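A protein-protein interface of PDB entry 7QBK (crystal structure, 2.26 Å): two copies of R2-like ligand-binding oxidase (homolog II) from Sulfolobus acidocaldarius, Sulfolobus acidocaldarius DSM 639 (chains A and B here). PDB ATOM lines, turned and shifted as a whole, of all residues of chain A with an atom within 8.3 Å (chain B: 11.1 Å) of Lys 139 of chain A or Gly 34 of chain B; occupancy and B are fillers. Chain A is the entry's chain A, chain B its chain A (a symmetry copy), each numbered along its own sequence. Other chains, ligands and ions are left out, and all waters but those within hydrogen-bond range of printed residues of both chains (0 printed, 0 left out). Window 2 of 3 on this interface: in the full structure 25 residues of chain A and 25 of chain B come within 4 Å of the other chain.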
ATOM      1  N   VAL A  79      -5.055  -8.201   8.591  1.00  0.00           N
ATOM      2  CA  VAL A  79      -3.958  -9.094   8.943  1.00  0.00           C
ATOM      3  C   VAL A  79      -4.035 -10.369   8.116  1.00  0.00           C
ATOM      4  O   VAL A  79      -3.003 -10.901   7.689  1.00  0.00           O
ATOM      5  CB  VAL A  79      -3.973  -9.387  10.456  1.00  0.00           C
ATOM      6  CG1 VAL A  79      -2.897 -10.393  10.818  1.00  0.00           C
ATOM      7  CG2 VAL A  79      -3.766  -8.101  11.238  1.00  0.00           C
ATOM      8  N   SER A  83      -0.638 -10.902   5.930  1.00  0.00           N
ATOM      9  CA  SER A  83       0.201 -12.019   6.351  1.00  0.00           C
ATOM     10  C   SER A  83       0.287 -13.081   5.263  1.00  0.00           C
ATOM     11  O   SER A  83       1.341 -13.699   5.078  1.00  0.00           O
ATOM     12  CB  SER A  83      -0.327 -12.617   7.657  1.00  0.00           C
ATOM     13  OG  SER A  83      -1.638 -13.127   7.491  1.00  0.00           O
ATOM     14  N   PHE A 129       5.617  -5.492   3.280  1.00  0.00           N
ATOM     15  CA  PHE A 129       4.497  -5.906   4.118  1.00  0.00           C
ATOM     16  C   PHE A 129       4.910  -6.034   5.577  1.00  0.00           C
ATOM     17  O   PHE A 129       4.123  -5.708   6.474  1.00  0.00           O
ATOM     18  CB  PHE A 129       3.907  -7.222   3.608  1.00  0.00           C
ATOM     19  CG  PHE A 129       3.185  -7.085   2.301  1.00  0.00           C
ATOM     20  CD1 PHE A 129       1.987  -6.397   2.230  1.00  0.00           C
ATOM     21  CD2 PHE A 129       3.710  -7.636   1.145  1.00  0.00           C
ATOM     22  CE1 PHE A 129       1.327  -6.257   1.024  1.00  0.00           C
ATOM     23  CE2 PHE A 129       3.052  -7.506  -0.058  1.00  0.00           C
ATOM     24  CZ  PHE A 129       1.859  -6.816  -0.120  1.00  0.00           C
ATOM     25  N   ARG A 130       6.138  -6.488   5.831  1.00  0.00           N
ATOM     26  CA  ARG A 130       6.625  -6.578   7.202  1.00  0.00           C
ATOM     27  C   ARG A 130       6.777  -5.203   7.842  1.00  0.00           C
ATOM     28  O   ARG A 130       6.553  -5.057   9.048  1.00  0.00           O
ATOM     29  CB  ARG A 130       7.951  -7.335   7.235  1.00  0.00           C
ATOM     30  CG  ARG A 130       7.978  -8.450   8.266  1.00  0.00           C
ATOM     31  CD  ARG A 130       9.327  -9.141   8.315  1.00  0.00           C
ATOM     32  NE  ARG A 130       9.447 -10.223   7.345  1.00  0.00           N
ATOM     33  CZ  ARG A 130       9.109 -11.483   7.584  1.00  0.00           C
ATOM     34  NH1 ARG A 130       8.575 -11.850   8.739  1.00  0.00           N
ATOM     35  NH2 ARG A 130       9.315 -12.401   6.644  1.00  0.00           N
ATOM     36  N   ARG A 131       7.156  -4.185   7.065  1.00  0.00           N
ATOM     37  CA  ARG A 131       7.240  -2.843   7.628  1.00  0.00           C
ATOM     38  C   ARG A 131       5.859  -2.286   7.942  1.00  0.00           C
ATOM     39  O   ARG A 131       5.698  -1.553   8.924  1.00  0.00           O
ATOM     40  CB  ARG A 131       7.991  -1.915   6.677  1.00  0.00           C
ATOM     41  CG  ARG A 131       9.457  -2.275   6.500  1.00  0.00           C
ATOM     42  CD  ARG A 131      10.144  -1.354   5.503  1.00  0.00           C
ATOM     43  NE  ARG A 131      10.796  -0.234   6.169  1.00  0.00           N
ATOM     44  CZ  ARG A 131      12.070  -0.224   6.536  1.00  0.00           C
ATOM     45  NH1 ARG A 131      12.868  -1.251   6.293  1.00  0.00           N
ATOM     46  NH2 ARG A 131      12.558   0.845   7.159  1.00  0.00           N
ATOM     47  N   PHE A 132       4.853  -2.634   7.138  1.00  0.00           N
ATOM     48  CA  PHE A 132       3.492  -2.193   7.423  1.00  0.00           C
ATOM     49  C   PHE A 132       2.937  -2.889   8.659  1.00  0.00           C
ATOM     50  O   PHE A 132       2.299  -2.255   9.503  1.00  0.00           O
ATOM     51  CB  PHE A 132       2.592  -2.441   6.215  1.00  0.00           C
ATOM     52  CG  PHE A 132       1.138  -2.175   6.484  1.00  0.00           C
ATOM     53  CD1 PHE A 132       0.607  -0.910   6.307  1.00  0.00           C
ATOM     54  CD2 PHE A 132       0.302  -3.194   6.919  1.00  0.00           C
ATOM     55  CE1 PHE A 132      -0.729  -0.662   6.561  1.00  0.00           C
ATOM     56  CE2 PHE A 132      -1.031  -2.954   7.173  1.00  0.00           C
ATOM     57  CZ  PHE A 132      -1.548  -1.688   6.994  1.00  0.00           C
ATOM     58  N   LEU A 133       3.148  -4.202   8.770  1.00  0.00           N
ATOM     59  CA  LEU A 133       2.712  -4.908   9.971  1.00  0.00           C
ATOM     60  C   LEU A 133       3.446  -4.406  11.206  1.00  0.00           C
ATOM     61  O   LEU A 133       2.861  -4.340  12.294  1.00  0.00           O
ATOM     62  CB  LEU A 133       2.912  -6.413   9.797  1.00  0.00           C
ATOM     63  CG  LEU A 133       1.981  -7.045   8.765  1.00  0.00           C
ATOM     64  CD1 LEU A 133       2.264  -8.529   8.607  1.00  0.00           C
ATOM     65  CD2 LEU A 133       0.535  -6.804   9.164  1.00  0.00           C
ATOM     66  N   ASP A 134       4.718  -4.039  11.051  1.00  0.00           N
ATOM     67  CA  ASP A 134       5.474  -3.470  12.159  1.00  0.00           C
ATOM     68  C   ASP A 134       4.971  -2.078  12.522  1.00  0.00           C
ATOM     69  O   ASP A 134       4.940  -1.715  13.703  1.00  0.00           O
ATOM     70  CB  ASP A 134       6.959  -3.420  11.802  1.00  0.00           C
ATOM     71  CG  ASP A 134       7.819  -2.920  12.942  1.00  0.00           C
ATOM     72  OD1 ASP A 134       8.104  -3.716  13.867  1.00  0.00           O
ATOM     73  OD2 ASP A 134       8.219  -1.735  12.913  1.00  0.00           O
ATOM     74  N   ALA A 135       4.560  -1.293  11.525  1.00  0.00           N
ATOM     75  CA  ALA A 135       4.102   0.068  11.793  1.00  0.00           C
ATOM     76  C   ALA A 135       2.764   0.078  12.522  1.00  0.00           C
ATOM     77  O   ALA A 135       2.521   0.947  13.368  1.00  0.00           O
ATOM     78  CB  ALA A 135       3.994   0.860  10.490  1.00  0.00           C
ATOM     79  N   VAL A 136       1.874  -0.869  12.204  1.00  0.00           N
ATOM     80  CA  VAL A 136       0.567  -0.919  12.851  1.00  0.00           C
ATOM     81  C   VAL A 136       0.597  -1.675  14.172  1.00  0.00           C
ATOM     82  O   VAL A 136      -0.437  -1.767  14.848  1.00  0.00           O
ATOM     83  CB  VAL A 136      -0.494  -1.545  11.922  1.00  0.00           C
ATOM     84  CG1 VAL A 136      -0.649  -0.707  10.656  1.00  0.00           C
ATOM     85  CG2 VAL A 136      -0.123  -2.972  11.580  1.00  0.00           C
ATOM     86  N   GLY A 137       1.744  -2.221  14.560  1.00  0.00           N
ATOM     87  CA  GLY A 137       1.856  -2.910  15.832  1.00  0.00           C
ATOM     88  C   GLY A 137       1.261  -4.301  15.861  1.00  0.00           C
ATOM     89  O   GLY A 137       0.563  -4.652  16.821  1.00  0.00           O
ATOM     90  N   VAL A 138       1.517  -5.107  14.834  1.00  0.00           N
ATOM     91  CA  VAL A 138       1.007  -6.471  14.739  1.00  0.00           C
ATOM     92  C   VAL A 138       2.187  -7.425  14.853  1.00  0.00           C
ATOM     93  O   VAL A 138       3.150  -7.326  14.082  1.00  0.00           O
ATOM     94  CB  VAL A 138       0.238  -6.699  13.429  1.00  0.00           C
ATOM     95  CG1 VAL A 138       0.004  -8.185  13.195  1.00  0.00           C
ATOM     96  CG2 VAL A 138      -1.083  -5.947  13.452  1.00  0.00           C
ATOM     97  N   LYS A 139       2.116  -8.344  15.809  1.00  0.00           N
ATOM     98  CA  LYS A 139       3.200  -9.298  16.018  1.00  0.00           C
ATOM     99  C   LYS A 139       2.696 -10.735  15.930  1.00  0.00           C
ATOM    100  O   LYS A 139       3.061 -11.475  15.017  1.00  0.00           O
ATOM    101  CB  LYS A 139       3.869  -9.056  17.371  1.00  0.00           C
ATOM    102  CG  LYS A 139       4.388  -7.640  17.568  1.00  0.00           C
ATOM    103  CD  LYS A 139       5.042  -7.489  18.933  1.00  0.00           C
ATOM    104  CE  LYS A 139       5.491  -6.061  19.185  1.00  0.00           C
ATOM    105  NZ  LYS A 139       6.498  -5.607  18.189  1.00  0.00           N
ATOM    106  N   GLY B  34       6.791  -6.888  14.219  1.00  0.00           N
ATOM    107  CA  GLY B  34       7.569  -7.160  15.414  1.00  0.00           C
ATOM    108  C   GLY B  34       9.064  -7.208  15.162  1.00  0.00           C
ATOM    109  O   GLY B  34       9.747  -8.143  15.582  1.00  0.00           O
ATOM    110  N   ILE B  35       9.574  -6.191  14.476  1.00  0.00           N
ATOM    111  CA  ILE B  35      10.986  -6.114  14.120  1.00  0.00           C
ATOM    112  C   ILE B  35      11.720  -5.303  15.179  1.00  0.00           C
ATOM    113  O   ILE B  35      11.248  -4.242  15.601  1.00  0.00           O
ATOM    114  CB  ILE B  35      11.167  -5.491  12.726  1.00  0.00           C
ATOM    115  CG1 ILE B  35      10.410  -6.307  11.675  1.00  0.00           C
ATOM    116  CG2 ILE B  35      12.641  -5.386  12.367  1.00  0.00           C
ATOM    117  CD1 ILE B  35      10.510  -5.744  10.273  1.00  0.00           C
ATOM    118  N   ASP B  36      12.871  -5.807  15.615  1.00  0.00           N
ATOM    119  CA  ASP B  36      13.759  -5.066  16.510  1.00  0.00           C
ATOM    120  C   ASP B  36      14.765  -4.325  15.641  1.00  0.00           C
ATOM    121  O   ASP B  36      15.723  -4.916  15.136  1.00  0.00           O
ATOM    122  CB  ASP B  36      14.443  -6.007  17.496  1.00  0.00           C
ATOM    123  CG  ASP B  36      15.313  -5.272  18.504  1.00  0.00           C
ATOM    124  OD1 ASP B  36      15.312  -4.021  18.508  1.00  0.00           O
ATOM    125  OD2 ASP B  36      16.006  -5.946  19.293  1.00  0.00           O
ATOM    126  N   TRP B  37      14.545  -3.023  15.458  1.00  0.00           N
ATOM    127  CA  TRP B  37      15.434  -2.217  14.632  1.00  0.00           C
ATOM    128  C   TRP B  37      16.742  -1.867  15.332  1.00  0.00           C
ATOM    129  O   TRP B  37      17.686  -1.433  14.661  1.00  0.00           O
ATOM    130  CB  TRP B  37      14.719  -0.936  14.190  1.00  0.00           C
ATOM    131  CG  TRP B  37      13.427  -1.206  13.480  1.00  0.00           C
ATOM    132  CD1 TRP B  37      12.180  -1.244  14.035  1.00  0.00           C
ATOM    133  CD2 TRP B  37      13.255  -1.494  12.086  1.00  0.00           C
ATOM    134  NE1 TRP B  37      11.244  -1.531  13.072  1.00  0.00           N
ATOM    135  CE2 TRP B  37      11.877  -1.689  11.868  1.00  0.00           C
ATOM    136  CE3 TRP B  37      14.131  -1.604  11.003  1.00  0.00           C
ATOM    137  CZ2 TRP B  37      11.354  -1.988  10.611  1.00  0.00           C
ATOM    138  CZ3 TRP B  37      13.610  -1.901   9.754  1.00  0.00           C
ATOM    139  CH2 TRP B  37      12.235  -2.089   9.571  1.00  0.00           C
ATOM    140  N   SER B  38      16.826  -2.048  16.650  1.00  0.00           N
ATOM    141  CA  SER B  38      18.062  -1.794  17.377  1.00  0.00           C
ATOM    142  C   SER B  38      19.036  -2.964  17.319  1.00  0.00           C
ATOM    143  O   SER B  38      20.156  -2.837  17.823  1.00  0.00           O
ATOM    144  CB  SER B  38      17.754  -1.467  18.838  1.00  0.00           C
ATOM    145  OG  SER B  38      17.189  -2.587  19.494  1.00  0.00           O
ATOM    146  N   LEU B  39      18.635  -4.092  16.737  1.00  0.00           N
ATOM    147  CA  LEU B  39      19.521  -5.242  16.632  1.00  0.00           C
ATOM    148  C   LEU B  39      20.623  -4.969  15.616  1.00  0.00           C
ATOM    149  O   LEU B  39      20.444  -4.210  14.659  1.00  0.00           O
ATOM    150  CB  LEU B  39      18.735  -6.487  16.225  1.00  0.00           C
ATOM    151  CG  LEU B  39      19.124  -7.799  16.907  1.00  0.00           C
ATOM    152  CD1 LEU B  39      18.872  -7.691  18.398  1.00  0.00           C
ATOM    153  CD2 LEU B  39      18.353  -8.963  16.314  1.00  0.00           C
ATOM    154  N   MET B  42      19.988  -5.311  11.780  1.00  0.00           N
ATOM    155  CA  MET B  42      19.190  -4.236  11.200  1.00  0.00           C
ATOM    156  C   MET B  42      20.004  -2.962  11.031  1.00  0.00           C
ATOM    157  O   MET B  42      19.719  -2.159  10.133  1.00  0.00           O
ATOM    158  CB  MET B  42      17.953  -3.976  12.061  1.00  0.00           C
ATOM    159  CG  MET B  42      17.014  -5.171  12.154  1.00  0.00           C
ATOM    160  SD  MET B  42      16.689  -5.956  10.559  1.00  0.00           S
ATOM    161  CE  MET B  42      15.800  -4.662   9.705  1.00  0.00           C
ATOM    162  N   GLY B 107      12.882 -18.504  13.319  1.00  0.00           N
ATOM    163  CA  GLY B 107      12.183 -17.261  13.578  1.00  0.00           C
ATOM    164  C   GLY B 107      13.077 -16.067  13.819  1.00  0.00           C
ATOM    165  O   GLY B 107      12.683 -15.141  14.536  1.00  0.00           O
ATOM    166  N   ARG B 108      14.276 -16.056  13.237  1.00  0.00           N
ATOM    167  CA  ARG B 108      15.204 -14.937  13.388  1.00  0.00           C
ATOM    168  C   ARG B 108      15.020 -13.999  12.200  1.00  0.00           C
ATOM    169  O   ARG B 108      15.770 -14.019  11.225  1.00  0.00           O
ATOM    170  CB  ARG B 108      16.633 -15.447  13.509  1.00  0.00           C
ATOM    171  CG  ARG B 108      16.808 -16.424  14.648  1.00  0.00           C
ATOM    172  CD  ARG B 108      18.247 -16.854  14.787  1.00  0.00           C
ATOM    173  NE  ARG B 108      18.436 -17.720  15.944  1.00  0.00           N
ATOM    174  CZ  ARG B 108      18.618 -17.282  17.181  1.00  0.00           C
ATOM    175  NH1 ARG B 108      18.612 -15.990  17.464  1.00  0.00           N
ATOM    176  NH2 ARG B 108      18.812 -18.163  18.158  1.00  0.00           N
ATOM    177  N   VAL B 109      13.988 -13.155  12.304  1.00  0.00           N
ATOM    178  CA  VAL B 109      13.564 -12.330  11.178  1.00  0.00           C
ATOM    179  C   VAL B 109      14.614 -11.279  10.842  1.00  0.00           C
ATOM    180  O   VAL B 109      14.858 -10.982   9.666  1.00  0.00           O
ATOM    181  CB  VAL B 109      12.194 -11.694  11.482  1.00  0.00           C
ATOM    182  CG1 VAL B 109      11.815 -10.684  10.409  1.00  0.00           C
ATOM    183  CG2 VAL B 109      11.125 -12.774  11.598  1.00  0.00           C
ATOM    184  N   GLU B 110      15.251 -10.700  11.861  1.00  0.00           N
ATOM    185  CA  GLU B 110      16.265  -9.680  11.613  1.00  0.00           C
ATOM    186  C   GLU B 110      17.436 -10.245  10.820  1.00  0.00           C
ATOM    187  O   GLU B 110      17.886  -9.640   9.840  1.00  0.00           O
ATOM    188  CB  GLU B 110      16.747  -9.084  12.937  1.00  0.00           C
ATOM    189  CG  GLU B 110      15.698  -8.261  13.661  1.00  0.00           C
ATOM    190  CD  GLU B 110      14.741  -9.109  14.470  1.00  0.00           C
ATOM    191  OE1 GLU B 110      14.953 -10.337  14.554  1.00  0.00           O
ATOM    192  OE2 GLU B 110      13.776  -8.547  15.028  1.00  0.00           O
ATOM    193  N   GLU B 111      17.937 -11.414  11.219  1.00  0.00           N
ATOM    194  CA  GLU B 111      19.066 -11.998  10.503  1.00  0.00           C
ATOM    195  C   GLU B 111      18.661 -12.514   9.127  1.00  0.00           C
ATOM    196  O   GLU B 111      19.497 -12.556   8.217  1.00  0.00           O
ATOM    197  CB  GLU B 111      19.700 -13.110  11.336  1.00  0.00           C
ATOM    198  CG  GLU B 111      20.275 -12.622  12.656  1.00  0.00           C
ATOM    199  CD  GLU B 111      20.761 -13.757  13.531  1.00  0.00           C
ATOM    200  OE1 GLU B 111      20.909 -14.882  13.014  1.00  0.00           O
ATOM    201  OE2 GLU B 111      20.995 -13.524  14.736  1.00  0.00           O
ATOM    202  N   MET B 113      16.355 -10.991   7.218  1.00  0.00           N
ATOM    203  CA  MET B 113      16.233  -9.805   6.381  1.00  0.00           C
ATOM    204  C   MET B 113      17.596  -9.342   5.874  1.00  0.00           C
ATOM    205  O   MET B 113      17.713  -8.888   4.732  1.00  0.00           O
ATOM    206  CB  MET B 113      15.531  -8.682   7.148  1.00  0.00           C
ATOM    207  CG  MET B 113      14.034  -8.895   7.328  1.00  0.00           C
ATOM    208  SD  MET B 113      13.204  -7.482   8.068  1.00  0.00           S
ATOM    209  CE  MET B 113      13.499  -6.224   6.832  1.00  0.00           C
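The side-chain carboxylate of Asp 134 of chain A lies within hydrogen-bond range of the backbone NH of Ile 35 of chain B.
OD2 of Asp 134 of chain A lies within hydrogen-bond range of NE1 of Trp 37 of chain B.
OD1 of Asp 134 of chain A is in hydrogen-bond range of N of Gly 34 of chain B, 3.5 Å away.
O of Leu 133 of chain A sits at hydrogen-bond distance from N of Val 138 of chain A, at 3.0 Å.
Among the printed residues, merely in contact across the chains: Arg 130 of chain A with Val 109 of chain B, Arg 131 of chain A with Trp 37 of chain B, Val 138 of chain A with Gly 34 of chain B and Lys 139 of chain A with Gly 34 of chain B.
Along chain A the printed residues that touch a printed residue of chain B span positions 130 to 139.
Printed residues of chain B that touch a printed residue of chain A: Gly 34, Ile 35, Trp 37 and Val 109.
Among the printed residues, 7 pairs touch across the chains.
No position is printed for both chains.
Of chain A, only Asp 134, Val 138 and Lys 139 come within 4 Å of Gly 34 of chain B.
Of the printed residues of chain B, Val 138 of chain A touches Gly 34 (3.7 Å).
Printed residues of chain A within 4 Å of Trp 37 of chain B: Arg 131 and Asp 134.
Of the printed residues of chain B, Arg 130 of chain A touches Val 109.
Of the printed residues of chain A, Ile 35 of chain B touches Asp 134 (2.9 Å).
The nearest residue of chain B that does not touch Lys 139 of chain A is Ile 35 of chain B (4.9 Å).
The nearest residue of chain A that does not touch Gly 34 of chain B is Leu 133 of chain A (5.1 Å).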
